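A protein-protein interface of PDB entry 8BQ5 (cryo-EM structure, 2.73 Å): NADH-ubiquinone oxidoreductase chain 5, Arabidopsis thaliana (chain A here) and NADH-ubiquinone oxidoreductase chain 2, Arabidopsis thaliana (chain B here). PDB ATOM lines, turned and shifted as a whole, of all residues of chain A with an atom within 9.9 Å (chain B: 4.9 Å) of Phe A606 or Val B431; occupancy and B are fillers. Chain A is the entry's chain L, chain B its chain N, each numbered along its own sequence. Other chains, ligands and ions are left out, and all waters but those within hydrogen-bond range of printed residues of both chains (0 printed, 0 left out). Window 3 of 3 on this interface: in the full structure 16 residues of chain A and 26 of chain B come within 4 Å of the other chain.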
ATOM      1  N   GLY A 598      -9.684  -3.638 -26.289  1.00  0.00           N
ATOM      2  CA  GLY A 598     -10.774  -3.441 -27.209  1.00  0.00           C
ATOM      3  C   GLY A 598     -10.965  -4.631 -28.124  1.00  0.00           C
ATOM      4  O   GLY A 598     -10.784  -5.784 -27.726  1.00  0.00           O
ATOM      5  N   PRO A 599     -11.311  -4.364 -29.384  1.00  0.00           N
ATOM      6  CA  PRO A 599     -11.711  -5.463 -30.282  1.00  0.00           C
ATOM      7  C   PRO A 599     -10.638  -6.519 -30.491  1.00  0.00           C
ATOM      8  O   PRO A 599     -10.973  -7.699 -30.644  1.00  0.00           O
ATOM      9  CB  PRO A 599     -12.068  -4.750 -31.595  1.00  0.00           C
ATOM     10  CG  PRO A 599     -11.920  -3.295 -31.353  1.00  0.00           C
ATOM     11  CD  PRO A 599     -11.216  -3.065 -30.066  1.00  0.00           C
ATOM     12  N   TYR A 600      -9.360  -6.138 -30.522  1.00  0.00           N
ATOM     13  CA  TYR A 600      -8.310  -7.143 -30.650  1.00  0.00           C
ATOM     14  C   TYR A 600      -8.225  -8.012 -29.402  1.00  0.00           C
ATOM     15  O   TYR A 600      -8.218  -9.245 -29.489  1.00  0.00           O
ATOM     16  CB  TYR A 600      -6.964  -6.478 -30.921  1.00  0.00           C
ATOM     17  CG  TYR A 600      -5.880  -7.463 -31.290  1.00  0.00           C
ATOM     18  CD1 TYR A 600      -5.935  -8.167 -32.484  1.00  0.00           C
ATOM     19  CD2 TYR A 600      -4.814  -7.706 -30.435  1.00  0.00           C
ATOM     20  CE1 TYR A 600      -4.953  -9.072 -32.824  1.00  0.00           C
ATOM     21  CE2 TYR A 600      -3.824  -8.612 -30.767  1.00  0.00           C
ATOM     22  CZ  TYR A 600      -3.901  -9.292 -31.964  1.00  0.00           C
ATOM     23  OH  TYR A 600      -2.924 -10.196 -32.306  1.00  0.00           O
ATOM     24  N   GLY A 601      -8.145  -7.380 -28.232  1.00  0.00           N
ATOM     25  CA  GLY A 601      -8.058  -8.138 -26.995  1.00  0.00           C
ATOM     26  C   GLY A 601      -9.344  -8.864 -26.655  1.00  0.00           C
ATOM     27  O   GLY A 601      -9.314  -9.987 -26.149  1.00  0.00           O
ATOM     28  N   ILE A 602     -10.489  -8.226 -26.910  1.00  0.00           N
ATOM     29  CA  ILE A 602     -11.778  -8.837 -26.595  1.00  0.00           C
ATOM     30  C   ILE A 602     -12.002 -10.083 -27.441  1.00  0.00           C
ATOM     31  O   ILE A 602     -12.496 -11.105 -26.949  1.00  0.00           O
ATOM     32  CB  ILE A 602     -12.913  -7.812 -26.776  1.00  0.00           C
ATOM     33  CG1 ILE A 602     -13.044  -6.940 -25.528  1.00  0.00           C
ATOM     34  CG2 ILE A 602     -14.229  -8.504 -27.105  1.00  0.00           C
ATOM     35  CD1 ILE A 602     -13.519  -5.537 -25.811  1.00  0.00           C
ATOM     36  N   SER A 603     -11.650 -10.018 -28.725  1.00  0.00           N
ATOM     37  CA  SER A 603     -11.814 -11.177 -29.597  1.00  0.00           C
ATOM     38  C   SER A 603     -10.954 -12.348 -29.135  1.00  0.00           C
ATOM     39  O   SER A 603     -11.408 -13.499 -29.133  1.00  0.00           O
ATOM     40  CB  SER A 603     -11.480 -10.792 -31.037  1.00  0.00           C
ATOM     41  OG  SER A 603     -10.117 -11.037 -31.333  1.00  0.00           O
ATOM     42  N   TYR A 604      -9.715 -12.069 -28.725  1.00  0.00           N
ATOM     43  CA  TYR A 604      -8.798 -13.126 -28.309  1.00  0.00           C
ATOM     44  C   TYR A 604      -9.318 -13.864 -27.079  1.00  0.00           C
ATOM     45  O   TYR A 604      -9.365 -15.102 -27.053  1.00  0.00           O
ATOM     46  CB  TYR A 604      -7.411 -12.521 -28.053  1.00  0.00           C
ATOM     47  CG  TYR A 604      -6.477 -13.341 -27.181  1.00  0.00           C
ATOM     48  CD1 TYR A 604      -6.551 -13.286 -25.792  1.00  0.00           C
ATOM     49  CD2 TYR A 604      -5.517 -14.165 -27.751  1.00  0.00           C
ATOM     50  CE1 TYR A 604      -5.702 -14.033 -25.001  1.00  0.00           C
ATOM     51  CE2 TYR A 604      -4.662 -14.915 -26.965  1.00  0.00           C
ATOM     52  CZ  TYR A 604      -4.759 -14.845 -25.592  1.00  0.00           C
ATOM     53  OH  TYR A 604      -3.910 -15.587 -24.807  1.00  0.00           O
ATOM     54  N   THR A 605      -9.718 -13.117 -26.046  1.00  0.00           N
ATOM     55  CA  THR A 605     -10.123 -13.760 -24.800  1.00  0.00           C
ATOM     56  C   THR A 605     -11.423 -14.528 -24.975  1.00  0.00           C
ATOM     57  O   THR A 605     -11.596 -15.603 -24.392  1.00  0.00           O
ATOM     58  CB  THR A 605     -10.259 -12.732 -23.676  1.00  0.00           C
ATOM     59  OG1 THR A 605     -10.969 -13.319 -22.580  1.00  0.00           O
ATOM     60  CG2 THR A 605     -11.026 -11.517 -24.146  1.00  0.00           C
ATOM     61  N   PHE A 606     -12.350 -14.001 -25.775  1.00  0.00           N
ATOM     62  CA  PHE A 606     -13.603 -14.711 -25.976  1.00  0.00           C
ATOM     63  C   PHE A 606     -13.416 -15.935 -26.860  1.00  0.00           C
ATOM     64  O   PHE A 606     -14.092 -16.947 -26.657  1.00  0.00           O
ATOM     65  CB  PHE A 606     -14.655 -13.766 -26.547  1.00  0.00           C
ATOM     66  CG  PHE A 606     -15.473 -13.093 -25.490  1.00  0.00           C
ATOM     67  CD1 PHE A 606     -16.419 -13.806 -24.776  1.00  0.00           C
ATOM     68  CD2 PHE A 606     -15.276 -11.759 -25.186  1.00  0.00           C
ATOM     69  CE1 PHE A 606     -17.166 -13.197 -23.792  1.00  0.00           C
ATOM     70  CE2 PHE A 606     -16.021 -11.144 -24.202  1.00  0.00           C
ATOM     71  CZ  PHE A 606     -16.968 -11.862 -23.506  1.00  0.00           C
ATOM     72  N   ARG A 607     -12.489 -15.879 -27.817  1.00  0.00           N
ATOM     73  CA  ARG A 607     -12.135 -17.083 -28.560  1.00  0.00           C
ATOM     74  C   ARG A 607     -11.567 -18.149 -27.631  1.00  0.00           C
ATOM     75  O   ARG A 607     -11.932 -19.327 -27.721  1.00  0.00           O
ATOM     76  CB  ARG A 607     -11.134 -16.747 -29.662  1.00  0.00           C
ATOM     77  CG  ARG A 607     -10.813 -17.918 -30.567  1.00  0.00           C
ATOM     78  CD  ARG A 607      -9.830 -17.516 -31.644  1.00  0.00           C
ATOM     79  NE  ARG A 607     -10.290 -16.342 -32.374  1.00  0.00           N
ATOM     80  CZ  ARG A 607      -9.492 -15.390 -32.838  1.00  0.00           C
ATOM     81  NH1 ARG A 607      -8.182 -15.443 -32.665  1.00  0.00           N
ATOM     82  NH2 ARG A 607     -10.022 -14.361 -33.491  1.00  0.00           N
ATOM     83  N   ARG A 608     -10.671 -17.752 -26.722  1.00  0.00           N
ATOM     84  CA  ARG A 608     -10.095 -18.726 -25.796  1.00  0.00           C
ATOM     85  C   ARG A 608     -11.151 -19.282 -24.842  1.00  0.00           C
ATOM     86  O   ARG A 608     -11.142 -20.477 -24.527  1.00  0.00           O
ATOM     87  CB  ARG A 608      -8.937 -18.098 -25.021  1.00  0.00           C
ATOM     88  CG  ARG A 608      -7.770 -17.636 -25.891  1.00  0.00           C
ATOM     89  CD  ARG A 608      -6.755 -18.747 -26.150  1.00  0.00           C
ATOM     90  NE  ARG A 608      -7.219 -19.750 -27.105  1.00  0.00           N
ATOM     91  CZ  ARG A 608      -7.532 -19.513 -28.373  1.00  0.00           C
ATOM     92  NH1 ARG A 608      -7.405 -18.309 -28.906  1.00  0.00           N
ATOM     93  NH2 ARG A 608      -7.970 -20.515 -29.129  1.00  0.00           N
ATOM     94  N   LEU A 609     -12.069 -18.432 -24.374  1.00  0.00           N
ATOM     95  CA  LEU A 609     -13.142 -18.900 -23.501  1.00  0.00           C
ATOM     96  C   LEU A 609     -14.074 -19.865 -24.226  1.00  0.00           C
ATOM     97  O   LEU A 609     -14.492 -20.878 -23.652  1.00  0.00           O
ATOM     98  CB  LEU A 609     -13.937 -17.716 -22.954  1.00  0.00           C
ATOM     99  CG  LEU A 609     -13.292 -16.840 -21.881  1.00  0.00           C
ATOM    100  CD1 LEU A 609     -14.279 -15.786 -21.410  1.00  0.00           C
ATOM    101  CD2 LEU A 609     -12.814 -17.687 -20.714  1.00  0.00           C
ATOM    102  N   ALA A 610     -14.431 -19.555 -25.475  1.00  0.00           N
ATOM    103  CA  ALA A 610     -15.262 -20.464 -26.256  1.00  0.00           C
ATOM    104  C   ALA A 610     -14.557 -21.794 -26.472  1.00  0.00           C
ATOM    105  O   ALA A 610     -15.177 -22.859 -26.365  1.00  0.00           O
ATOM    106  CB  ALA A 610     -15.628 -19.821 -27.592  1.00  0.00           C
ATOM    107  N   GLU A 611     -13.259 -21.749 -26.777  1.00  0.00           N
ATOM    108  CA  GLU A 611     -12.451 -22.962 -26.850  1.00  0.00           C
ATOM    109  C   GLU A 611     -12.563 -23.780 -25.569  1.00  0.00           C
ATOM    110  O   GLU A 611     -12.856 -24.981 -25.606  1.00  0.00           O
ATOM    111  CB  GLU A 611     -10.995 -22.576 -27.111  1.00  0.00           C
ATOM    112  CG  GLU A 611     -10.045 -23.739 -27.282  1.00  0.00           C
ATOM    113  CD  GLU A 611      -8.632 -23.297 -27.587  1.00  0.00           C
ATOM    114  OE1 GLU A 611      -8.389 -22.073 -27.625  1.00  0.00           O
ATOM    115  OE2 GLU A 611      -7.766 -24.173 -27.794  1.00  0.00           O
ATOM    116  N   ARG A 612     -12.346 -23.134 -24.420  1.00  0.00           N
ATOM    117  CA  ARG A 612     -12.354 -23.848 -23.146  1.00  0.00           C
ATOM    118  C   ARG A 612     -13.717 -24.466 -22.857  1.00  0.00           C
ATOM    119  O   ARG A 612     -13.803 -25.604 -22.385  1.00  0.00           O
ATOM    120  CB  ARG A 612     -11.947 -22.905 -22.015  1.00  0.00           C
ATOM    121  CG  ARG A 612     -10.544 -22.341 -22.143  1.00  0.00           C
ATOM    122  CD  ARG A 612      -9.491 -23.428 -22.061  1.00  0.00           C
ATOM    123  NE  ARG A 612      -9.533 -24.129 -20.783  1.00  0.00           N
ATOM    124  CZ  ARG A 612      -8.966 -23.687 -19.670  1.00  0.00           C
ATOM    125  NH1 ARG A 612      -8.315 -22.536 -19.636  1.00  0.00           N
ATOM    126  NH2 ARG A 612      -9.054 -24.418 -18.562  1.00  0.00           N
ATOM    127  N   ILE A 613     -14.792 -23.725 -23.123  1.00  0.00           N
ATOM    128  CA  ILE A 613     -16.134 -24.244 -22.874  1.00  0.00           C
ATOM    129  C   ILE A 613     -16.453 -25.393 -23.824  1.00  0.00           C
ATOM    130  O   ILE A 613     -17.138 -26.353 -23.453  1.00  0.00           O
ATOM    131  CB  ILE A 613     -17.168 -23.108 -22.976  1.00  0.00           C
ATOM    132  CG1 ILE A 613     -17.021 -22.153 -21.788  1.00  0.00           C
ATOM    133  CG2 ILE A 613     -18.582 -23.665 -23.066  1.00  0.00           C
ATOM    134  CD1 ILE A 613     -17.940 -22.456 -20.627  1.00  0.00           C
ATOM    135  N   SER A 614     -15.966 -25.316 -25.064  1.00  0.00           N
ATOM    136  CA  SER A 614     -16.244 -26.366 -26.038  1.00  0.00           C
ATOM    137  C   SER A 614     -15.649 -27.699 -25.603  1.00  0.00           C
ATOM    138  O   SER A 614     -16.260 -28.754 -25.798  1.00  0.00           O
ATOM    139  CB  SER A 614     -15.711 -25.957 -27.411  1.00  0.00           C
ATOM    140  OG  SER A 614     -15.685 -27.056 -28.303  1.00  0.00           O
ATOM    141  N   LEU B 307     -21.176 -18.886 -25.437  1.00  0.00           N
ATOM    142  CA  LEU B 307     -19.774 -19.202 -25.706  1.00  0.00           C
ATOM    143  C   LEU B 307     -19.639 -20.467 -26.551  1.00  0.00           C
ATOM    144  O   LEU B 307     -18.879 -20.505 -27.532  1.00  0.00           O
ATOM    145  CB  LEU B 307     -19.008 -19.338 -24.392  1.00  0.00           C
ATOM    146  CG  LEU B 307     -18.749 -18.024 -23.652  1.00  0.00           C
ATOM    147  CD1 LEU B 307     -18.164 -18.296 -22.280  1.00  0.00           C
ATOM    148  CD2 LEU B 307     -17.838 -17.114 -24.457  1.00  0.00           C
ATOM    149  N   MET B 310     -20.555 -19.859 -30.062  1.00  0.00           N
ATOM    150  CA  MET B 310     -19.440 -19.175 -30.703  1.00  0.00           C
ATOM    151  C   MET B 310     -18.349 -20.151 -31.127  1.00  0.00           C
ATOM    152  O   MET B 310     -17.675 -19.927 -32.138  1.00  0.00           O
ATOM    153  CB  MET B 310     -18.873 -18.116 -29.762  1.00  0.00           C
ATOM    154  CG  MET B 310     -17.753 -17.285 -30.350  1.00  0.00           C
ATOM    155  SD  MET B 310     -17.877 -15.551 -29.877  1.00  0.00           S
ATOM    156  CE  MET B 310     -17.221 -15.619 -28.212  1.00  0.00           C
ATOM    157  N   LEU B 427     -26.303  -6.965 -17.381  1.00  0.00           N
ATOM    158  CA  LEU B 427     -24.961  -7.053 -17.952  1.00  0.00           C
ATOM    159  C   LEU B 427     -24.763  -8.364 -18.706  1.00  0.00           C
ATOM    160  O   LEU B 427     -24.235  -8.376 -19.829  1.00  0.00           O
ATOM    161  CB  LEU B 427     -23.925  -6.921 -16.837  1.00  0.00           C
ATOM    162  CG  LEU B 427     -22.440  -6.878 -17.192  1.00  0.00           C
ATOM    163  CD1 LEU B 427     -22.199  -6.104 -18.480  1.00  0.00           C
ATOM    164  CD2 LEU B 427     -21.653  -6.275 -16.041  1.00  0.00           C
ATOM    165  N   VAL B 428     -25.170  -9.478 -18.095  1.00  0.00           N
ATOM    166  CA  VAL B 428     -25.036 -10.777 -18.744  1.00  0.00           C
ATOM    167  C   VAL B 428     -25.848 -10.806 -20.028  1.00  0.00           C
ATOM    168  O   VAL B 428     -25.388 -11.308 -21.059  1.00  0.00           O
ATOM    169  CB  VAL B 428     -25.449 -11.906 -17.780  1.00  0.00           C
ATOM    170  CG1 VAL B 428     -25.477 -13.234 -18.509  1.00  0.00           C
ATOM    171  CG2 VAL B 428     -24.493 -11.972 -16.602  1.00  0.00           C
ATOM    172  N   GLY B 429     -27.062 -10.257 -19.990  1.00  0.00           N
ATOM    173  CA  GLY B 429     -27.877 -10.196 -21.189  1.00  0.00           C
ATOM    174  C   GLY B 429     -27.228  -9.391 -22.297  1.00  0.00           C
ATOM    175  O   GLY B 429     -27.242  -9.802 -23.455  1.00  0.00           O
ATOM    176  N   VAL B 430     -26.639  -8.242 -21.956  1.00  0.00           N
ATOM    177  CA  VAL B 430     -25.987  -7.413 -22.970  1.00  0.00           C
ATOM    178  C   VAL B 430     -24.839  -8.178 -23.623  1.00  0.00           C
ATOM    179  O   VAL B 430     -24.747  -8.272 -24.858  1.00  0.00           O
ATOM    180  CB  VAL B 430     -25.497  -6.092 -22.349  1.00  0.00           C
ATOM    181  CG1 VAL B 430     -24.465  -5.425 -23.248  1.00  0.00           C
ATOM    182  CG2 VAL B 430     -26.664  -5.158 -22.081  1.00  0.00           C
ATOM    183  N   VAL B 431     -23.960  -8.754 -22.799  1.00  0.00           N
ATOM    184  CA  VAL B 431     -22.780  -9.433 -23.333  1.00  0.00           C
ATOM    185  C   VAL B 431     -23.189 -10.644 -24.169  1.00  0.00           C
ATOM    186  O   VAL B 431     -22.667 -10.868 -25.271  1.00  0.00           O
ATOM    187  CB  VAL B 431     -21.824  -9.827 -22.194  1.00  0.00           C
ATOM    188  CG1 VAL B 431     -20.585 -10.498 -22.757  1.00  0.00           C
ATOM    189  CG2 VAL B 431     -21.437  -8.596 -21.384  1.00  0.00           C
ATOM    190  N   THR B 432     -24.132 -11.442 -23.660  1.00  0.00           N
ATOM    191  CA  THR B 432     -24.573 -12.624 -24.394  1.00  0.00           C
ATOM    192  C   THR B 432     -25.305 -12.253 -25.674  1.00  0.00           C
ATOM    193  O   THR B 432     -25.160 -12.949 -26.682  1.00  0.00           O
ATOM    194  CB  THR B 432     -25.462 -13.501 -23.512  1.00  0.00           C
ATOM    195  OG1 THR B 432     -26.557 -12.728 -23.006  1.00  0.00           O
ATOM    196  CG2 THR B 432     -24.662 -14.069 -22.355  1.00  0.00           C
ATOM    197  N   SER B 433     -26.083 -11.169 -25.665  1.00  0.00           N
ATOM    198  CA  SER B 433     -26.749 -10.724 -26.882  1.00  0.00           C
ATOM    199  C   SER B 433     -25.738 -10.327 -27.945  1.00  0.00           C
ATOM    200  O   SER B 433     -25.906 -10.651 -29.126  1.00  0.00           O
ATOM    201  CB  SER B 433     -27.683  -9.556 -26.570  1.00  0.00           C
ATOM    202  OG  SER B 433     -28.896 -10.013 -26.002  1.00  0.00           O
ATOM    203  N   VAL B 434     -24.670  -9.635 -27.546  1.00  0.00           N
ATOM    204  CA  VAL B 434     -23.660  -9.235 -28.522  1.00  0.00           C
ATOM    205  C   VAL B 434     -22.920 -10.455 -29.073  1.00  0.00           C
ATOM    206  O   VAL B 434     -22.686 -10.564 -30.287  1.00  0.00           O
ATOM    207  CB  VAL B 434     -22.705  -8.207 -27.892  1.00  0.00           C
ATOM    208  CG1 VAL B 434     -21.484  -8.008 -28.758  1.00  0.00           C
ATOM    209  CG2 VAL B 434     -23.438  -6.900 -27.692  1.00  0.00           C
ATOM    210  N   ILE B 435     -22.558 -11.400 -28.198  1.00  0.00           N
ATOM    211  CA  ILE B 435     -21.897 -12.625 -28.655  1.00  0.00           C
ATOM    212  C   ILE B 435     -22.796 -13.391 -29.620  1.00  0.00           C
ATOM    213  O   ILE B 435     -22.342 -13.901 -30.660  1.00  0.00           O
ATOM    214  CB  ILE B 435     -21.507 -13.497 -27.447  1.00  0.00           C
ATOM    215  CG1 ILE B 435     -20.427 -12.816 -26.611  1.00  0.00           C
ATOM    216  CG2 ILE B 435     -21.045 -14.873 -27.903  1.00  0.00           C
ATOM    217  CD1 ILE B 435     -20.335 -13.360 -25.211  1.00  0.00           C
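Among the printed residues, merely in contact across the chains: Phe A606 with Leu B307, Phe A606 with Met B310, Phe A606 with Val B431, Phe A606 with Ile B435 and Ala A610 with Leu B307.
Of the printed residues of chain B, Ala A610 touches Leu B307 (3.3 Å). Glu A611 touches none of the printed residues of chain B. Ile A613 touches none of the printed residues of chain B. Of the printed residues of chain A, Leu B307 touches Phe A606 and Ala A610. Of the printed residues of chain A, Met B310 touches Phe A606. No residue of chain A comes within 4 Å of Val B430. No residue of chain A comes within 4 Å of Thr B432. No residue of chain A comes within 4 Å of Val B434. Of the printed residues of chain A, Ile B435 touches Phe A606 (3.5 Å). The nearest residue of chain A that does not touch Val B431 is Ile A602 (8.0 Å).
Of the 11 printed residues of chain B, 4 touch a printed residue of chain A. Hydrophobic or aromatic side chains of chain B that line the printed part of chain A: Leu B307, Met B310, Val B431 and Ile B435. Along chain B the printed residues that touch a printed residue of chain A span positions 307 to 435. Of the 17 printed residues of chain A, 2 touch a printed residue of chain B. Printed residues of chain A that touch a printed residue of chain B: Phe A606 and Ala A610. Hydrophobic or aromatic side chains of chain A within 4 Å of the printed part of chain B: Phe A606 and Ala A610. Among the printed residues, 5 pairs touch across the chains. Among the printed residues, no Asp or Glu carboxylate lies within 4 Å of a Lys or Arg side-chain nitrogen of the other chain.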
